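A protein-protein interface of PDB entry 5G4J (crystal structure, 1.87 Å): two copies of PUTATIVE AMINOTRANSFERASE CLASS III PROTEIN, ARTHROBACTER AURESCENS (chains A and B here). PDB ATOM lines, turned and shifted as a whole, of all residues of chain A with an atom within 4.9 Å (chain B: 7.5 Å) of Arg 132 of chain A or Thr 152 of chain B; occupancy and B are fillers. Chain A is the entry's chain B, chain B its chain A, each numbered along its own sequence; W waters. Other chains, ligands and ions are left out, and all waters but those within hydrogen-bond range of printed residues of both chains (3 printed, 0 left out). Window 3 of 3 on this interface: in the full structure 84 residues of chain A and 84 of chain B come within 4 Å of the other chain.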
ATOM      1  N   GLU A 125       3.387 -10.354  -8.956  1.00  0.00           N
ATOM      2  CA  GLU A 125       3.627 -10.523 -10.371  1.00  0.00           C
ATOM      3  C   GLU A 125       4.994 -10.064 -10.702  1.00  0.00           C
ATOM      4  O   GLU A 125       5.759 -10.761 -11.444  1.00  0.00           O
ATOM      5  CB  GLU A 125       2.598  -9.718 -11.185  1.00  0.00           C
ATOM      6  CG  GLU A 125       2.781  -9.739 -12.693  1.00  0.00           C
ATOM      7  CD  GLU A 125       2.449 -11.018 -13.393  1.00  0.00           C
ATOM      8  OE1 GLU A 125       1.906 -11.962 -12.768  1.00  0.00           O
ATOM      9  OE2 GLU A 125       2.717 -11.086 -14.645  1.00  0.00           O
ATOM     10  N   LEU A 128       7.759 -12.439  -9.194  1.00  0.00           N
ATOM     11  CA  LEU A 128       8.003 -13.589 -10.021  1.00  0.00           C
ATOM     12  C   LEU A 128       8.786 -13.300 -11.278  1.00  0.00           C
ATOM     13  O   LEU A 128       9.545 -14.183 -11.735  1.00  0.00           O
ATOM     14  CB  LEU A 128       6.693 -14.339 -10.372  1.00  0.00           C
ATOM     15  CG  LEU A 128       5.892 -15.006  -9.280  1.00  0.00           C
ATOM     16  CD1 LEU A 128       4.676 -15.611  -9.989  1.00  0.00           C
ATOM     17  CD2 LEU A 128       6.679 -16.058  -8.578  1.00  0.00           C
ATOM     18  N   ARG A 129       8.518 -12.162 -11.911  1.00  0.00           N
ATOM     19  CA  ARG A 129       9.159 -11.751 -13.109  1.00  0.00           C
ATOM     20  C   ARG A 129      10.659 -11.458 -12.892  1.00  0.00           C
ATOM     21  O   ARG A 129      11.497 -11.911 -13.685  1.00  0.00           O
ATOM     22  CB  ARG A 129       8.436 -10.546 -13.728  1.00  0.00           C
ATOM     23  CG  ARG A 129       8.943 -10.061 -15.064  1.00  0.00           C
ATOM     24  CD  ARG A 129       8.061  -8.920 -15.621  1.00  0.00           C
ATOM     25  NE  ARG A 129       8.664  -8.452 -16.838  1.00  0.00           N
ATOM     26  CZ  ARG A 129       8.604  -7.227 -17.339  1.00  0.00           C
ATOM     27  NH1 ARG A 129       7.847  -6.261 -16.803  1.00  0.00           N
ATOM     28  NH2 ARG A 129       9.317  -6.968 -18.391  1.00  0.00           N
ATOM     29  N   ILE A 130      10.960 -10.683 -11.844  1.00  0.00           N
ATOM     30  CA  ILE A 130      12.373 -10.421 -11.415  1.00  0.00           C
ATOM     31  C   ILE A 130      13.028 -11.773 -11.199  1.00  0.00           C
ATOM     32  O   ILE A 130      14.124 -11.979 -11.724  1.00  0.00           O
ATOM     33  CB  ILE A 130      12.434  -9.600 -10.102  1.00  0.00           C
ATOM     34  CG1 ILE A 130      11.926  -8.187 -10.337  1.00  0.00           C
ATOM     35  CG2 ILE A 130      13.879  -9.554  -9.569  1.00  0.00           C
ATOM     36  CD1 ILE A 130      11.629  -7.436  -9.055  1.00  0.00           C
ATOM     37  N   ALA A 131      12.368 -12.718 -10.519  1.00  0.00           N
ATOM     38  CA  ALA A 131      13.022 -13.985 -10.193  1.00  0.00           C
ATOM     39  C   ALA A 131      13.296 -14.843 -11.443  1.00  0.00           C
ATOM     40  O   ALA A 131      14.391 -15.445 -11.602  1.00  0.00           O
ATOM     41  CB  ALA A 131      12.260 -14.748  -9.179  1.00  0.00           C
ATOM     42  N   ARG A 132      12.318 -14.875 -12.348  1.00  0.00           N
ATOM     43  CA  ARG A 132      12.409 -15.655 -13.571  1.00  0.00           C
ATOM     44  C   ARG A 132      13.589 -15.141 -14.403  1.00  0.00           C
ATOM     45  O   ARG A 132      14.372 -15.964 -14.930  1.00  0.00           O
ATOM     46  CB  ARG A 132      11.076 -15.501 -14.370  1.00  0.00           C
ATOM     47  CG  ARG A 132      10.785 -16.526 -15.401  1.00  0.00           C
ATOM     48  CD  ARG A 132       9.467 -16.331 -16.133  1.00  0.00           C
ATOM     49  NE  ARG A 132       8.321 -16.236 -15.194  1.00  0.00           N
ATOM     50  CZ  ARG A 132       7.622 -15.143 -14.905  1.00  0.00           C
ATOM     51  NH1 ARG A 132       7.870 -13.967 -15.505  1.00  0.00           N
ATOM     52  NH2 ARG A 132       6.587 -15.240 -14.050  1.00  0.00           N
ATOM     53  N   GLN A 133      13.683 -13.829 -14.591  1.00  0.00           N
ATOM     54  CA  GLN A 133      14.726 -13.268 -15.344  1.00  0.00           C
ATOM     55  C   GLN A 133      16.106 -13.483 -14.706  1.00  0.00           C
ATOM     56  O   GLN A 133      17.074 -13.803 -15.399  1.00  0.00           O
ATOM     57  CB  GLN A 133      14.531 -11.805 -15.545  1.00  0.00           C
ATOM     58  CG  GLN A 133      13.317 -11.456 -16.403  1.00  0.00           C
ATOM     59  CD  GLN A 133      13.306 -10.008 -16.804  1.00  0.00           C
ATOM     60  OE1 GLN A 133      14.315  -9.292 -16.715  1.00  0.00           O
ATOM     61  NE2 GLN A 133      12.219  -9.603 -17.429  1.00  0.00           N
ATOM     62  N   HIS A 134      16.176 -13.325 -13.408  1.00  0.00           N
ATOM     63  CA  HIS A 134      17.431 -13.449 -12.697  1.00  0.00           C
ATOM     64  C   HIS A 134      17.948 -14.890 -12.718  1.00  0.00           C
ATOM     65  O   HIS A 134      19.137 -15.128 -12.966  1.00  0.00           O
ATOM     66  CB  HIS A 134      17.283 -12.999 -11.236  1.00  0.00           C
ATOM     67  CG  HIS A 134      18.475 -13.351 -10.398  1.00  0.00           C
ATOM     68  ND1 HIS A 134      19.638 -12.611 -10.434  1.00  0.00           N
ATOM     69  CD2 HIS A 134      18.699 -14.378  -9.532  1.00  0.00           C
ATOM     70  CE1 HIS A 134      20.527 -13.147  -9.603  1.00  0.00           C
ATOM     71  NE2 HIS A 134      19.988 -14.230  -9.062  1.00  0.00           N
ATOM     72  N   THR A 135      17.066 -15.836 -12.451  1.00  0.00           N
ATOM     73  CA  THR A 135      17.455 -17.218 -12.243  1.00  0.00           C
ATOM     74  C   THR A 135      17.676 -17.935 -13.545  1.00  0.00           C
ATOM     75  O   THR A 135      18.363 -18.938 -13.571  1.00  0.00           O
ATOM     76  CB  THR A 135      16.461 -17.997 -11.381  1.00  0.00           C
ATOM     77  OG1 THR A 135      15.214 -18.151 -12.071  1.00  0.00           O
ATOM     78  CG2 THR A 135      16.259 -17.403  -9.997  1.00  0.00           C
ATOM     79  N   GLY A 136      17.030 -17.478 -14.624  1.00  0.00           N
ATOM     80  CA  GLY A 136      16.992 -18.235 -15.863  1.00  0.00           C
ATOM     81  C   GLY A 136      16.171 -19.500 -15.784  1.00  0.00           C
ATOM     82  O   GLY A 136      16.158 -20.258 -16.719  1.00  0.00           O
ATOM     83  N   ASN A 137      15.357 -19.624 -14.748  1.00  0.00           N
ATOM     84  CA  ASN A 137      14.486 -20.760 -14.504  1.00  0.00           C
ATOM     85  C   ASN A 137      13.030 -20.307 -14.457  1.00  0.00           C
ATOM     86  O   ASN A 137      12.768 -19.121 -14.317  1.00  0.00           O
ATOM     87  CB  ASN A 137      14.820 -21.468 -13.143  1.00  0.00           C
ATOM     88  CG  ASN A 137      16.235 -22.027 -13.079  1.00  0.00           C
ATOM     89  OD1 ASN A 137      16.897 -22.075 -11.974  1.00  0.00           O
ATOM     90  ND2 ASN A 137      16.700 -22.481 -14.206  1.00  0.00           N
ATOM     91  N   THR A 138      12.093 -21.248 -14.549  1.00  0.00           N
ATOM     92  CA  THR A 138      10.653 -20.967 -14.432  1.00  0.00           C
ATOM     93  C   THR A 138       9.947 -21.668 -13.316  1.00  0.00           C
ATOM     94  O   THR A 138       8.814 -21.320 -12.998  1.00  0.00           O
ATOM     95  CB  THR A 138       9.922 -21.329 -15.726  1.00  0.00           C
ATOM     96  OG1 THR A 138      10.209 -22.692 -16.059  1.00  0.00           O
ATOM     97  CG2 THR A 138      10.403 -20.400 -16.858  1.00  0.00           C
ATOM     98  N   SER A 153      -0.018 -15.104 -14.560  1.00  0.00           N
ATOM     99  CA  SER A 153       1.087 -15.865 -13.965  1.00  0.00           C
ATOM    100  C   SER A 153       0.786 -16.367 -12.572  1.00  0.00           C
ATOM    101  O   SER A 153       1.172 -17.512 -12.214  1.00  0.00           O
ATOM    102  CB  SER A 153       2.419 -15.112 -14.106  1.00  0.00           C
ATOM    103  OG  SER A 153       2.665 -14.267 -12.984  1.00  0.00           O
ATOM    104  N   SER A 213      12.909 -21.401  -9.974  1.00  0.00           N
ATOM    105  CA  SER A 213      12.993 -19.938  -9.956  1.00  0.00           C
ATOM    106  C   SER A 213      12.734 -19.423  -8.544  1.00  0.00           C
ATOM    107  O   SER A 213      13.506 -18.620  -7.993  1.00  0.00           O
ATOM    108  CB  SER A 213      11.942 -19.310 -10.931  1.00  0.00           C
ATOM    109  OG  SER A 213      12.051 -17.914 -10.904  1.00  0.00           O
ATOM    110  N   GLU B 125      -3.977  -6.839 -18.387  1.00  0.00           N
ATOM    111  CA  GLU B 125      -3.709  -8.221 -17.923  1.00  0.00           C
ATOM    112  C   GLU B 125      -4.996  -9.044 -17.762  1.00  0.00           C
ATOM    113  O   GLU B 125      -5.116 -10.160 -18.320  1.00  0.00           O
ATOM    114  CB  GLU B 125      -3.000  -8.216 -16.563  1.00  0.00           C
ATOM    115  CG  GLU B 125      -2.698  -9.564 -15.965  1.00  0.00           C
ATOM    116  CD  GLU B 125      -1.602 -10.347 -16.662  1.00  0.00           C
ATOM    117  OE1 GLU B 125      -0.913  -9.819 -17.566  1.00  0.00           O
ATOM    118  OE2 GLU B 125      -1.396 -11.533 -16.235  1.00  0.00           O
ATOM    119  N   GLY B 149       1.541  -2.302 -21.041  1.00  0.00           N
ATOM    120  CA  GLY B 149       1.747  -2.528 -19.587  1.00  0.00           C
ATOM    121  C   GLY B 149       2.865  -3.410 -19.228  1.00  0.00           C
ATOM    122  O   GLY B 149       3.633  -3.886 -20.089  1.00  0.00           O
ATOM    123  N   ASN B 150       2.973  -3.697 -17.958  1.00  0.00           N
ATOM    124  CA  ASN B 150       4.249  -4.184 -17.380  1.00  0.00           C
ATOM    125  C   ASN B 150       4.241  -5.526 -16.651  1.00  0.00           C
ATOM    126  O   ASN B 150       5.176  -5.816 -15.863  1.00  0.00           O
ATOM    127  CB  ASN B 150       4.758  -3.079 -16.387  1.00  0.00           C
ATOM    128  CG  ASN B 150       3.757  -2.787 -15.322  1.00  0.00           C
ATOM    129  OD1 ASN B 150       3.087  -3.712 -14.824  1.00  0.00           O
ATOM    130  ND2 ASN B 150       3.624  -1.513 -14.954  1.00  0.00           N
ATOM    131  N   THR B 151       3.191  -6.316 -16.802  1.00  0.00           N
ATOM    132  CA  THR B 151       3.109  -7.656 -16.249  1.00  0.00           C
ATOM    133  C   THR B 151       3.922  -8.600 -17.127  1.00  0.00           C
ATOM    134  O   THR B 151       4.419  -8.195 -18.200  1.00  0.00           O
ATOM    135  CB  THR B 151       1.652  -8.185 -16.251  1.00  0.00           C
ATOM    136  OG1 THR B 151       1.158  -8.237 -17.612  1.00  0.00           O
ATOM    137  CG2 THR B 151       0.803  -7.277 -15.401  1.00  0.00           C
ATOM    138  N   THR B 152       4.059  -9.850 -16.697  1.00  0.00           N
ATOM    139  CA  THR B 152       4.745 -10.883 -17.531  1.00  0.00           C
ATOM    140  C   THR B 152       4.050 -11.099 -18.869  1.00  0.00           C
ATOM    141  O   THR B 152       4.666 -11.034 -19.934  1.00  0.00           O
ATOM    142  CB  THR B 152       4.877 -12.198 -16.785  1.00  0.00           C
ATOM    143  OG1 THR B 152       5.811 -11.961 -15.722  1.00  0.00           O
ATOM    144  CG2 THR B 152       5.455 -13.347 -17.716  1.00  0.00           C
ATOM    145  N   SER B 153       2.741 -11.285 -18.833  1.00  0.00           N
ATOM    146  CA  SER B 153       2.014 -11.548 -20.096  1.00  0.00           C
ATOM    147  C   SER B 153       2.097 -10.364 -21.025  1.00  0.00           C
ATOM    148  O   SER B 153       2.161 -10.543 -22.254  1.00  0.00           O
ATOM    149  CB  SER B 153       0.591 -12.088 -19.792  1.00  0.00           C
ATOM    150  OG  SER B 153      -0.359 -10.997 -19.603  1.00  0.00           O
ATOM    151  N   LEU B 154       2.112  -9.144 -20.478  1.00  0.00           N
ATOM    152  CA  LEU B 154       2.183  -7.932 -21.332  1.00  0.00           C
ATOM    153  C   LEU B 154       3.622  -7.711 -21.822  1.00  0.00           C
ATOM    154  O   LEU B 154       3.850  -7.294 -22.943  1.00  0.00           O
ATOM    155  CB  LEU B 154       1.645  -6.716 -20.616  1.00  0.00           C
ATOM    156  CG  LEU B 154       0.173  -6.788 -20.297  1.00  0.00           C
ATOM    157  CD1 LEU B 154      -0.244  -5.751 -19.271  1.00  0.00           C
ATOM    158  CD2 LEU B 154      -0.647  -6.676 -21.578  1.00  0.00           C
ATOM    159  N   ALA B 155       4.611  -8.066 -20.978  1.00  0.00           N
ATOM    160  CA  ALA B 155       6.013  -7.978 -21.454  1.00  0.00           C
ATOM    161  C   ALA B 155       6.246  -8.851 -22.695  1.00  0.00           C
ATOM    162  O   ALA B 155       6.975  -8.427 -23.588  1.00  0.00           O
ATOM    163  CB  ALA B 155       6.994  -8.388 -20.340  1.00  0.00           C
ATOM    164  N   GLU B 156       5.674 -10.066 -22.679  1.00  0.00           N
ATOM    165  CA  GLU B 156       5.824 -11.036 -23.774  1.00  0.00           C
ATOM    166  C   GLU B 156       5.218 -10.512 -25.097  1.00  0.00           C
ATOM    167  O   GLU B 156       5.575 -11.052 -26.159  1.00  0.00           O
ATOM    168  CB  GLU B 156       5.196 -12.362 -23.411  1.00  0.00           C
ATOM    169  CG  GLU B 156       5.864 -13.018 -22.253  1.00  0.00           C
ATOM    170  CD  GLU B 156       5.172 -14.282 -21.774  1.00  0.00           C
ATOM    171  OE1 GLU B 156       4.011 -14.528 -22.118  1.00  0.00           O
ATOM    172  OE2 GLU B 156       5.778 -14.958 -20.929  1.00  0.00           O
ATOM    173  N   ILE B 157       4.343  -9.478 -25.069  1.00  0.00           N
ATOM    174  CA  ILE B 157       3.756  -8.939 -26.279  1.00  0.00           C
ATOM    175  C   ILE B 157       4.290  -7.564 -26.620  1.00  0.00           C
ATOM    176  O   ILE B 157       3.893  -6.964 -27.590  1.00  0.00           O
ATOM    177  CB  ILE B 157       2.219  -8.929 -26.208  1.00  0.00           C
ATOM    178  CG1 ILE B 157       1.659  -7.774 -25.350  1.00  0.00           C
ATOM    179  CG2 ILE B 157       1.710 -10.257 -25.703  1.00  0.00           C
ATOM    180  CD1 ILE B 157       0.146  -7.672 -25.351  1.00  0.00           C
ATOM    181  N   THR B 158       5.223  -7.047 -25.802  1.00  0.00           N
ATOM    182  CA  THR B 158       5.691  -5.667 -25.954  1.00  0.00           C
ATOM    183  C   THR B 158       6.689  -5.425 -27.102  1.00  0.00           C
ATOM    184  O   THR B 158       7.685  -6.091 -27.149  1.00  0.00           O
ATOM    185  CB  THR B 158       6.297  -5.212 -24.601  1.00  0.00           C
ATOM    186  OG1 THR B 158       5.298  -5.220 -23.564  1.00  0.00           O
ATOM    187  CG2 THR B 158       6.862  -3.897 -24.691  1.00  0.00           C
ATOM    188  N   HIS B 164      13.321  -7.653 -21.264  1.00  0.00           N
ATOM    189  CA  HIS B 164      14.206  -8.792 -21.340  1.00  0.00           C
ATOM    190  C   HIS B 164      13.536  -9.950 -22.047  1.00  0.00           C
ATOM    191  O   HIS B 164      14.141 -10.707 -22.767  1.00  0.00           O
ATOM    192  CB  HIS B 164      14.522  -9.245 -19.929  1.00  0.00           C
ATOM    193  CG  HIS B 164      15.612 -10.266 -19.833  1.00  0.00           C
ATOM    194  ND1 HIS B 164      15.375 -11.594 -19.542  1.00  0.00           N
ATOM    195  CD2 HIS B 164      16.956 -10.132 -19.968  1.00  0.00           C
ATOM    196  CE1 HIS B 164      16.537 -12.226 -19.459  1.00  0.00           C
ATOM    197  NE2 HIS B 164      17.507 -11.361 -19.707  1.00  0.00           N
ATOM    198  N   GLU B 165      12.232 -10.110 -21.830  1.00  0.00           N
ATOM    199  CA  GLU B 165      11.477 -11.246 -22.461  1.00  0.00           C
ATOM    200  C   GLU B 165      11.552 -11.155 -24.008  1.00  0.00           C
ATOM    201  O   GLU B 165      11.290 -10.077 -24.566  1.00  0.00           O
ATOM    202  CB  GLU B 165      10.019 -11.174 -22.096  1.00  0.00           C
ATOM    203  CG  GLU B 165       9.800 -11.520 -20.615  1.00  0.00           C
ATOM    204  CD  GLU B 165       9.995 -10.376 -19.613  1.00  0.00           C
ATOM    205  OE1 GLU B 165      10.354  -9.222 -19.963  1.00  0.00           O
ATOM    206  OE2 GLU B 165       9.683 -10.644 -18.414  1.00  0.00           O
ATOM    207  N   HIS B 170       3.532 -16.753 -29.413  1.00  0.00           N
ATOM    208  CA  HIS B 170       2.131 -16.520 -29.617  1.00  0.00           C
ATOM    209  C   HIS B 170       1.752 -15.107 -30.058  1.00  0.00           C
ATOM    210  O   HIS B 170       0.552 -14.805 -30.173  1.00  0.00           O
ATOM    211  CB  HIS B 170       1.344 -16.859 -28.373  1.00  0.00           C
ATOM    212  CG  HIS B 170       1.698 -16.000 -27.196  1.00  0.00           C
ATOM    213  ND1 HIS B 170       2.932 -16.063 -26.567  1.00  0.00           N
ATOM    214  CD2 HIS B 170       1.039 -14.983 -26.624  1.00  0.00           C
ATOM    215  CE1 HIS B 170       2.949 -15.191 -25.562  1.00  0.00           C
ATOM    216  NE2 HIS B 170       1.833 -14.499 -25.605  1.00  0.00           N
HETATM  217  O   HOH W   1       1.080 -12.527 -16.186  1.00  0.00           O
HETATM  218  O   HOH W   2       5.060 -12.853 -13.192  1.00  0.00           O
HETATM  219  O   HOH W   3       9.492 -13.183 -17.774  1.00  0.00           O
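Water W3 lies within hydrogen-bond range of OE2 of Glu 165 of chain B (2.6 Å) and NH1 of Arg 132 of chain A (2.9 Å).
Water W1 lies within hydrogen-bond range of OE2 of Glu 125 of chain B (2.7 Å), OE2 of Glu 125 of chain A (2.7 Å), N of Ser 153 of chain A (3.2 Å) and N of Ser 153 of chain B (3.4 Å).
Water W2 lies within hydrogen-bond range of OG1 of Thr 152 of chain B (2.8 Å), OG of Ser 153 of chain A (2.8 Å), O of Glu 125 of chain A (2.8 Å) and NH2 of Arg 132 of chain A (3.0 Å).
The backbone carbonyl oxygen (O) of Asn 150 of chain B sits at hydrogen-bond distance from the guanidinium group (NH1) of Arg 129 of chain A (2.9 Å).
N of Thr 152 of chain B lies within hydrogen-bond range of OE2 of Glu 125 of chain A (2.7 Å).
NH1 of Arg 132 of chain A sits at hydrogen-bond distance from OG1 of Thr 152 of chain B (2.9 Å).
The side-chain carboxylate (OE2) of Glu 165 of chain B lies within salt-bridge range of the guanidinium group (NE) of Arg 129 of chain A, at 2.9 Å.
The side-chain carboxylate (OE2) of Glu 165 of chain B lies within hydrogen-bond range of the side-chain amide nitrogen (NE2) of Gln 133 of chain A.
Among the printed residues, pairs that only touch across the chains: Gln 133 of chain A with His 164 of chain B (3.2 Å), Arg 129 of chain A with Ala 155 of chain B (3.3 Å), Glu 125 of chain A with Thr 151 of chain B (3.5 Å) and Arg 129 of chain A with Thr 152 of chain B (3.6 Å).
Of the 14 printed residues of chain A, 4 touch a printed residue of chain B.
Of the 14 printed residues of chain B, 6 touch a printed residue of chain A.
Printed residues of chain B that touch a printed residue of chain A: Asn 150, Thr 151, Thr 152, Ala 155, His 164 and Glu 165.
Hydrophobic or aromatic side chains of chain B within 4 Å of the printed part of chain A: Ala 155 and His 164.
Positions printed for both chains: 125 and 153.
Of the 9 pairs that touch across the chains among the printed residues, none has its exchanged pair printed and touching as well.
No residue of chain B comes within 4 Å of Ala 131 of chain A.
Ser 213 of chain A touches none of the printed residues of chain B.
Printed residues of chain A within 4 Å of Asn 150 of chain B: Arg 129.
Printed residues of chain A within 4 Å of Thr 151 of chain B: Glu 125.
Thr 152 of chain B touches just these residues of chain A: Glu 125, Arg 129 and Arg 132.
Of the printed residues of chain A, Ala 155 of chain B touches Arg 129 (3.3 Å).
Of the printed residues of chain A, His 164 of chain B touches Gln 133 (3.2 Å).
The nearest residue of chain A that does not touch Thr 152 of chain B is Ser 153 of chain A (4.7 Å).
The side-chain carboxylate of Glu 125 of chain B lies within hydrogen-bond range of the side-chain hydroxyl of Thr 151 of chain B.
The side-chain hydroxyl (OG1) of Thr 151 of chain B lies within hydrogen-bond range of the backbone NH (N) of Leu 154 of chain B (3.2 Å).
OE1 of Glu 125 of chain A lies within hydrogen-bond range of OG of Ser 153 of chain A (2.4 Å).
N of Arg 132 of chain A sits at hydrogen-bond distance from OG of Ser 213 of chain A (3.4 Å).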
